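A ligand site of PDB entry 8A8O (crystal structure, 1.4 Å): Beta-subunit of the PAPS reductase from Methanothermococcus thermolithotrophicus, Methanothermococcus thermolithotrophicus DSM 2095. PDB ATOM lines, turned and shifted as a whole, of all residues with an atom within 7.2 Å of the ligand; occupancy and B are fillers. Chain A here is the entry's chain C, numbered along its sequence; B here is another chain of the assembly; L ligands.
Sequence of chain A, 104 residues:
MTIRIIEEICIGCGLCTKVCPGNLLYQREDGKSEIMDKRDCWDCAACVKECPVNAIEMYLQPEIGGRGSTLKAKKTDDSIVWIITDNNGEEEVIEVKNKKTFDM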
ATOM      1  N   THR A   2      20.301   6.977  10.676  1.00  0.00           N
ATOM      2  CA  THR A   2      20.920   6.095  11.688  1.00  0.00           C
ATOM      3  C   THR A   2      22.304   6.676  12.001  1.00  0.00           C
ATOM      4  O   THR A   2      22.675   7.741  11.484  1.00  0.00           O
ATOM      5  CB  THR A   2      20.960   4.630  11.227  1.00  0.00           C
ATOM      6  OG1 THR A   2      21.422   3.769  12.289  1.00  0.00           O
ATOM      7  CG2 THR A   2      21.862   4.431  10.013  1.00  0.00           C
ATOM      8  N   ILE A   3      23.067   5.986  12.838  1.00  0.00           N
ATOM      9  CA  ILE A   3      24.373   6.473  13.262  1.00  0.00           C
ATOM     10  C   ILE A   3      25.408   5.382  13.055  1.00  0.00           C
ATOM     11  O   ILE A   3      25.106   4.181  13.013  1.00  0.00           O
ATOM     12  CB  ILE A   3      24.398   6.967  14.733  1.00  0.00           C
ATOM     13  CG1 ILE A   3      24.066   5.830  15.691  1.00  0.00           C
ATOM     14  CG2 ILE A   3      23.456   8.125  14.906  1.00  0.00           C
ATOM     15  CD1 ILE A   3      25.258   5.212  16.365  1.00  0.00           C
ATOM     16  N   CYS A  16      28.348   8.103  25.400  1.00  0.00           N
ATOM     17  CA  CYS A  16      27.248   7.883  24.470  1.00  0.00           C
ATOM     18  C   CYS A  16      26.361   6.720  24.891  1.00  0.00           C
ATOM     19  O   CYS A  16      25.301   6.540  24.292  1.00  0.00           O
ATOM     20  CB  CYS A  16      27.802   7.595  23.082  1.00  0.00           C
ATOM     21  SG  CYS A  16      28.868   6.131  23.073  1.00  0.00           S
ATOM     22  N   VAL A  19      22.531   7.720  27.095  1.00  0.00           N
ATOM     23  CA  VAL A  19      21.573   8.705  26.609  1.00  0.00           C
ATOM     24  C   VAL A  19      20.457   8.156  25.731  1.00  0.00           C
ATOM     25  O   VAL A  19      19.373   8.757  25.651  1.00  0.00           O
ATOM     26  CB  VAL A  19      22.290   9.864  25.859  1.00  0.00           C
ATOM     27  CG1 VAL A  19      23.276  10.545  26.770  1.00  0.00           C
ATOM     28  CG2 VAL A  19      22.985   9.339  24.597  1.00  0.00           C
ATOM     29  N   CYS A  20      20.683   7.021  25.075  1.00  0.00           N
ATOM     30  CA  CYS A  20      19.798   6.602  23.977  1.00  0.00           C
ATOM     31  C   CYS A  20      18.412   6.218  24.470  1.00  0.00           C
ATOM     32  O   CYS A  20      18.299   5.328  25.335  1.00  0.00           O
ATOM     33  CB  CYS A  20      20.397   5.421  23.212  1.00  0.00           C
ATOM     34  SG  CYS A  20      19.357   4.874  21.830  1.00  0.00           S
ATOM     35  N   PRO A  21      17.347   6.820  23.941  1.00  0.00           N
ATOM     36  CA  PRO A  21      15.989   6.436  24.353  1.00  0.00           C
ATOM     37  C   PRO A  21      15.619   5.018  24.000  1.00  0.00           C
ATOM     38  O   PRO A  21      14.589   4.513  24.485  1.00  0.00           O
ATOM     39  CB  PRO A  21      15.089   7.416  23.590  1.00  0.00           C
ATOM     40  CG  PRO A  21      15.889   7.882  22.439  1.00  0.00           C
ATOM     41  CD  PRO A  21      17.331   7.881  22.918  1.00  0.00           C
ATOM     42  N   GLY A  22      16.371   4.373  23.112  1.00  0.00           N
ATOM     43  CA  GLY A  22      16.169   2.981  22.773  1.00  0.00           C
ATOM     44  C   GLY A  22      17.161   2.035  23.377  1.00  0.00           C
ATOM     45  O   GLY A  22      17.153   0.855  23.023  1.00  0.00           O
ATOM     46  N   ASN A  23      18.036   2.504  24.265  1.00  0.00           N
ATOM     47  CA  ASN A  23      19.080   1.659  24.852  1.00  0.00           C
ATOM     48  C   ASN A  23      19.981   1.001  23.798  1.00  0.00           C
ATOM     49  O   ASN A  23      20.474  -0.114  24.000  1.00  0.00           O
ATOM     50  CB  ASN A  23      18.506   0.546  25.744  1.00  0.00           C
ATOM     51  CG  ASN A  23      17.925   1.072  27.024  1.00  0.00           C
ATOM     52  OD1 ASN A  23      18.659   1.550  27.895  1.00  0.00           O
ATOM     53  ND2 ASN A  23      16.600   0.975  27.175  1.00  0.00           N
ATOM     54  N   LEU A  24      20.224   1.673  22.679  1.00  0.00           N
ATOM     55  CA  LEU A  24      20.846   0.982  21.555  1.00  0.00           C
ATOM     56  C   LEU A  24      22.357   0.913  21.650  1.00  0.00           C
ATOM     57  O   LEU A  24      22.965   0.114  20.922  1.00  0.00           O
ATOM     58  CB  LEU A  24      20.482   1.644  20.231  1.00  0.00           C
ATOM     59  CG  LEU A  24      18.993   1.632  19.841  1.00  0.00           C
ATOM     60  CD1 LEU A  24      18.784   2.364  18.517  1.00  0.00           C
ATOM     61  CD2 LEU A  24      18.493   0.212  19.741  1.00  0.00           C
ATOM     62  N   LEU A  25      22.993   1.733  22.485  1.00  0.00           N
ATOM     63  CA  LEU A  25      24.437   1.855  22.488  1.00  0.00           C
ATOM     64  C   LEU A  25      24.997   1.237  23.761  1.00  0.00           C
ATOM     65  O   LEU A  25      24.486   1.461  24.860  1.00  0.00           O
ATOM     66  CB  LEU A  25      24.883   3.307  22.385  1.00  0.00           C
ATOM     67  CG  LEU A  25      24.285   4.042  21.189  1.00  0.00           C
ATOM     68  CD1 LEU A  25      24.644   5.492  21.240  1.00  0.00           C
ATOM     69  CD2 LEU A  25      24.762   3.421  19.894  1.00  0.00           C
ATOM     70  N   ILE A  35      26.576  -0.061  18.449  1.00  0.00           N
ATOM     71  CA  ILE A  35      25.122   0.019  18.347  1.00  0.00           C
ATOM     72  C   ILE A  35      24.565  -1.384  18.159  1.00  0.00           C
ATOM     73  O   ILE A  35      25.139  -2.191  17.409  1.00  0.00           O
ATOM     74  CB  ILE A  35      24.693   0.974  17.214  1.00  0.00           C
ATOM     75  CG1 ILE A  35      23.172   1.117  17.146  1.00  0.00           C
ATOM     76  CG2 ILE A  35      25.229   0.514  15.863  1.00  0.00           C
ATOM     77  CD1 ILE A  35      22.703   2.409  16.504  1.00  0.00           C
ATOM     78  N   ASP A  37      21.657  -2.461  16.833  1.00  0.00           N
ATOM     79  CA  ASP A  37      21.092  -2.674  15.502  1.00  0.00           C
ATOM     80  C   ASP A  37      20.819  -1.288  14.921  1.00  0.00           C
ATOM     81  O   ASP A  37      19.951  -0.562  15.430  1.00  0.00           O
ATOM     82  CB  ASP A  37      19.809  -3.498  15.555  1.00  0.00           C
ATOM     83  CG  ASP A  37      19.377  -4.018  14.188  1.00  0.00           C
ATOM     84  OD1 ASP A  37      19.642  -3.334  13.168  1.00  0.00           O
ATOM     85  OD2 ASP A  37      18.782  -5.129  14.108  1.00  0.00           O
ATOM     86  N   LYS A  38      21.593  -0.900  13.911  1.00  0.00           N
ATOM     87  CA  LYS A  38      21.444   0.418  13.303  1.00  0.00           C
ATOM     88  C   LYS A  38      20.032   0.642  12.756  1.00  0.00           C
ATOM     89  O   LYS A  38      19.592   1.791  12.647  1.00  0.00           O
ATOM     90  CB  LYS A  38      22.489   0.608  12.199  1.00  0.00           C
ATOM     91  CG  LYS A  38      22.326  -0.316  11.024  1.00  0.00           C
ATOM     92  CD  LYS A  38      23.457  -0.166  10.004  1.00  0.00           C
ATOM     93  CE  LYS A  38      23.296  -1.147   8.858  1.00  0.00           C
ATOM     94  NZ  LYS A  38      24.421  -1.074   7.892  1.00  0.00           N
ATOM     95  N   ASP A  40      17.303   0.211  14.197  1.00  0.00           N
ATOM     96  CA  ASP A  40      16.381   0.632  15.246  1.00  0.00           C
ATOM     97  C   ASP A  40      16.598   2.058  15.676  1.00  0.00           C
ATOM     98  O   ASP A  40      15.929   2.518  16.605  1.00  0.00           O
ATOM     99  CB  ASP A  40      16.476  -0.313  16.441  1.00  0.00           C
ATOM    100  CG  ASP A  40      15.818  -1.658  16.171  1.00  0.00           C
ATOM    101  OD1 ASP A  40      14.935  -1.728  15.292  1.00  0.00           O
ATOM    102  OD2 ASP A  40      16.218  -2.634  16.819  1.00  0.00           O
ATOM    103  N   CYS A  41      17.518   2.784  15.026  1.00  0.00           N
ATOM    104  CA  CYS A  41      17.801   4.149  15.422  1.00  0.00           C
ATOM    105  C   CYS A  41      16.701   5.096  14.967  1.00  0.00           C
ATOM    106  O   CYS A  41      16.203   5.006  13.838  1.00  0.00           O
ATOM    107  CB  CYS A  41      19.153   4.574  14.812  1.00  0.00           C
ATOM    108  SG  CYS A  41      19.658   6.269  15.174  1.00  0.00           S
ATOM    109  N   TRP A  42      16.306   6.006  15.861  1.00  0.00           N
ATOM    110  CA  TRP A  42      15.294   7.030  15.599  1.00  0.00           C
ATOM    111  C   TRP A  42      15.888   8.328  15.062  1.00  0.00           C
ATOM    112  O   TRP A  42      15.146   9.254  14.722  1.00  0.00           O
ATOM    113  CB  TRP A  42      14.539   7.314  16.917  1.00  0.00           C
ATOM    114  CG  TRP A  42      13.266   8.073  16.832  1.00  0.00           C
ATOM    115  CD1 TRP A  42      12.428   8.181  15.739  1.00  0.00           C
ATOM    116  CD2 TRP A  42      12.661   8.836  17.872  1.00  0.00           C
ATOM    117  NE1 TRP A  42      11.345   8.952  16.069  1.00  0.00           N
ATOM    118  CE2 TRP A  42      11.471   9.368  17.368  1.00  0.00           C
ATOM    119  CE3 TRP A  42      13.014   9.110  19.193  1.00  0.00           C
ATOM    120  CZ2 TRP A  42      10.626  10.177  18.133  1.00  0.00           C
ATOM    121  CZ3 TRP A  42      12.183   9.914  19.958  1.00  0.00           C
ATOM    122  CH2 TRP A  42      11.005  10.440  19.424  1.00  0.00           C
ATOM    123  N   ASP A  43      17.214   8.424  14.988  1.00  0.00           N
ATOM    124  CA  ASP A  43      17.895   9.643  14.551  1.00  0.00           C
ATOM    125  C   ASP A  43      17.589  10.828  15.463  1.00  0.00           C
ATOM    126  O   ASP A  43      17.435  11.960  15.004  1.00  0.00           O
ATOM    127  CB  ASP A  43      17.609  10.001  13.099  1.00  0.00           C
ATOM    128  CG  ASP A  43      18.283   9.055  12.117  1.00  0.00           C
ATOM    129  OD1 ASP A  43      19.512   8.858  12.241  1.00  0.00           O
ATOM    130  OD2 ASP A  43      17.572   8.457  11.280  1.00  0.00           O
ATOM    131  N   CYS A  44      17.507  10.590  16.779  1.00  0.00           N
ATOM    132  CA  CYS A  44      17.261  11.671  17.713  1.00  0.00           C
ATOM    133  C   CYS A  44      18.501  12.536  17.950  1.00  0.00           C
ATOM    134  O   CYS A  44      18.374  13.668  18.422  1.00  0.00           O
ATOM    135  CB  CYS A  44      16.750  11.094  19.033  1.00  0.00           C
ATOM    136  SG  CYS A  44      17.999  10.356  20.080  1.00  0.00           S
ATOM    137  N   ALA A  45      19.692  12.012  17.615  1.00  0.00           N
ATOM    138  CA  ALA A  45      20.982  12.702  17.681  1.00  0.00           C
ATOM    139  C   ALA A  45      21.511  12.853  19.103  1.00  0.00           C
ATOM    140  O   ALA A  45      22.511  13.547  19.302  1.00  0.00           O
ATOM    141  CB  ALA A  45      20.953  14.065  16.989  1.00  0.00           C
ATOM    142  N   ALA A  46      20.882  12.231  20.093  1.00  0.00           N
ATOM    143  CA  ALA A  46      21.356  12.422  21.456  1.00  0.00           C
ATOM    144  C   ALA A  46      22.783  11.924  21.607  1.00  0.00           C
ATOM    145  O   ALA A  46      23.627  12.592  22.218  1.00  0.00           O
ATOM    146  CB  ALA A  46      20.430  11.711  22.447  1.00  0.00           C
ATOM    147  N   CYS A  47      23.079  10.745  21.039  1.00  0.00           N
ATOM    148  CA  CYS A  47      24.431  10.175  21.123  1.00  0.00           C
ATOM    149  C   CYS A  47      25.430  11.041  20.359  1.00  0.00           C
ATOM    150  O   CYS A  47      26.533  11.301  20.860  1.00  0.00           O
ATOM    151  CB  CYS A  47      24.407   8.749  20.567  1.00  0.00           C
ATOM    152  SG  CYS A  47      23.833   8.622  18.852  1.00  0.00           S
ATOM    153  N   VAL A  48      25.041  11.522  19.177  1.00  0.00           N
ATOM    154  CA  VAL A  48      25.918  12.350  18.358  1.00  0.00           C
ATOM    155  C   VAL A  48      26.421  13.544  19.149  1.00  0.00           C
ATOM    156  O   VAL A  48      27.603  13.897  19.093  1.00  0.00           O
ATOM    157  CB  VAL A  48      25.164  12.795  17.083  1.00  0.00           C
ATOM    158  CG1 VAL A  48      26.032  13.721  16.243  1.00  0.00           C
ATOM    159  CG2 VAL A  48      24.695  11.593  16.251  1.00  0.00           C
ATOM    160  N   ILE A  56      30.906   9.736  16.584  1.00  0.00           N
ATOM    161  CA  ILE A  56      29.582   9.282  16.166  1.00  0.00           C
ATOM    162  C   ILE A  56      29.110  10.219  15.085  1.00  0.00           C
ATOM    163  O   ILE A  56      29.117  11.450  15.266  1.00  0.00           O
ATOM    164  CB  ILE A  56      28.593   9.254  17.344  1.00  0.00           C
ATOM    165  CG1 ILE A  56      29.141   8.375  18.459  1.00  0.00           C
ATOM    166  CG2 ILE A  56      27.249   8.753  16.855  1.00  0.00           C
ATOM    167  CD1 ILE A  56      28.159   8.092  19.564  1.00  0.00           C
ATOM    168  N   MET A  58      25.861  10.769  12.186  1.00  0.00           N
ATOM    169  CA  MET A  58      24.543  10.397  11.697  1.00  0.00           C
ATOM    170  C   MET A  58      24.603  10.453  10.186  1.00  0.00           C
ATOM    171  O   MET A  58      25.234  11.349   9.604  1.00  0.00           O
ATOM    172  CB  MET A  58      23.487  11.343  12.262  1.00  0.00           C
ATOM    173  CG  MET A  58      22.101  11.140  11.682  1.00  0.00           C
ATOM    174  SD  MET A  58      20.860  12.268  12.348  1.00  0.00           S
ATOM    175  CE  MET A  58      20.868  11.775  14.075  1.00  0.00           C
ATOM    176  N   ARG B  45      17.196  11.779  28.361  1.00  0.00           N
ATOM    177  CA  ARG B  45      16.685  11.931  27.012  1.00  0.00           C
ATOM    178  C   ARG B  45      15.468  11.074  26.683  1.00  0.00           C
ATOM    179  O   ARG B  45      15.009  11.089  25.537  1.00  0.00           O
ATOM    180  CB  ARG B  45      17.781  11.611  25.971  1.00  0.00           C
ATOM    181  CG  ARG B  45      18.883  12.656  25.903  1.00  0.00           C
ATOM    182  CD  ARG B  45      18.417  13.867  25.131  1.00  0.00           C
ATOM    183  NE  ARG B  45      19.484  14.846  24.964  1.00  0.00           N
ATOM    184  CZ  ARG B  45      19.357  16.005  24.329  1.00  0.00           C
ATOM    185  NH1 ARG B  45      18.217  16.353  23.764  1.00  0.00           N
ATOM    186  NH2 ARG B  45      20.392  16.829  24.280  1.00  0.00           N
ATOM    187  N   ALA B  50      13.120  13.202  23.141  1.00  0.00           N
ATOM    188  CA  ALA B  50      14.551  12.938  23.018  1.00  0.00           C
ATOM    189  C   ALA B  50      15.231  13.854  22.029  1.00  0.00           C
ATOM    190  O   ALA B  50      16.357  14.317  22.279  1.00  0.00           O
ATOM    191  CB  ALA B  50      14.764  11.487  22.599  1.00  0.00           C
ATOM    192  N   PRO B 209       9.765   5.311  18.521  1.00  0.00           N
ATOM    193  CA  PRO B 209       9.702   3.856  18.282  1.00  0.00           C
ATOM    194  C   PRO B 209       9.945   3.020  19.533  1.00  0.00           C
ATOM    195  O   PRO B 209       9.831   1.799  19.466  1.00  0.00           O
ATOM    196  CB  PRO B 209      10.814   3.617  17.253  1.00  0.00           C
ATOM    197  CG  PRO B 209      11.773   4.765  17.455  1.00  0.00           C
ATOM    198  CD  PRO B 209      10.954   5.945  17.936  1.00  0.00           C
ATOM    199  N   PHE B 210      10.280   3.663  20.655  1.00  0.00           N
ATOM    200  CA  PHE B 210      10.560   2.983  21.924  1.00  0.00           C
ATOM    201  C   PHE B 210       9.416   3.101  22.913  1.00  0.00           C
ATOM    202  O   PHE B 210       9.518   2.564  24.020  1.00  0.00           O
ATOM    203  CB  PHE B 210      11.855   3.548  22.490  1.00  0.00           C
ATOM    204  CG  PHE B 210      12.937   3.654  21.434  1.00  0.00           C
ATOM    205  CD1 PHE B 210      13.380   2.511  20.782  1.00  0.00           C
ATOM    206  CD2 PHE B 210      13.469   4.873  21.084  1.00  0.00           C
ATOM    207  CE1 PHE B 210      14.350   2.575  19.800  1.00  0.00           C
ATOM    208  CE2 PHE B 210      14.466   4.946  20.117  1.00  0.00           C
ATOM    209  CZ  PHE B 210      14.890   3.813  19.472  1.00  0.00           C
HETATM  210 FE1  LIG L   1      19.123   8.619  19.115  1.00  0.00          FE
HETATM  211 FE2  LIG L   1      19.878   6.195  20.040  1.00  0.00          FE
HETATM  212 FE3  LIG L   1      21.753   7.807  18.947  1.00  0.00          FE
HETATM  213 FE4  LIG L   1      19.850   6.607  17.388  1.00  0.00          FE
HETATM  214  S1  LIG L   1      21.497   5.511  18.580  1.00  0.00           S
HETATM  215  S2  LIG L   1      20.467   8.874  17.313  1.00  0.00           S
HETATM  216  S3  LIG L   1      18.052   6.569  18.687  1.00  0.00           S
HETATM  217  S4  LIG L   1      20.633   8.201  20.838  1.00  0.00           S
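Merely in contact with the ligand: Ile 3 (3.9 Å), Pro 21 (3.9 Å), Ile 35 (3.9 Å), Asp 43 (3.9 Å) and Ala 46 (3.9 Å).
Of the 28 residues printed, 11 come within 4 Å of the ligand.
The nearest printed residue that does not touch the ligand is Leu 25 (4.1 Å).
The side-chain sulfur of Cys 44 lies close to the backbone NH of Ala 46 (3.4 Å).
SG of Cys 20 sits close to N of Asn 23 (3.6 Å).
SG of Cys 41 lies close to N of Asp 43, at 3.3 Å.
SG of Cys 20 sits close to N of Gly 22, at 3.3 Å.
The side-chain carboxylate (OD1) of Asp 43 lies within hydrogen-bond range of the backbone NH (N) of Thr 2 (2.6 Å).
N of Leu 24 lies close to SG of Cys 20 (3.4 Å).
An iron atom (FE1) of the ligand is bound by the side-chain sulfur of Cys 44.
The side-chain sulfur (SG) of Cys 47 is bound to an iron atom (FE3) of the ligand, 2.2 Å away.
An iron atom (FE4) of the ligand is bound by the side-chain sulfur (SG) of Cys 41 (2.2 Å).
The backbone NH (N) of Ala 45 of chain A lies close to a sulfur (S2) of the ligand (3.2 Å).
N of Cys 47 lies close to S4 of the ligand.
The side-chain sulfur of Cys 20 is bound to an iron atom (FE2) of the ligand (2.3 Å).
The backbone NH (N) of Cys 44 sits close to a sulfur (S2) of the ligand.
A sulfur (S3) of the ligand lies close to the backbone NH (N) of Trp 42 (3.4 Å).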
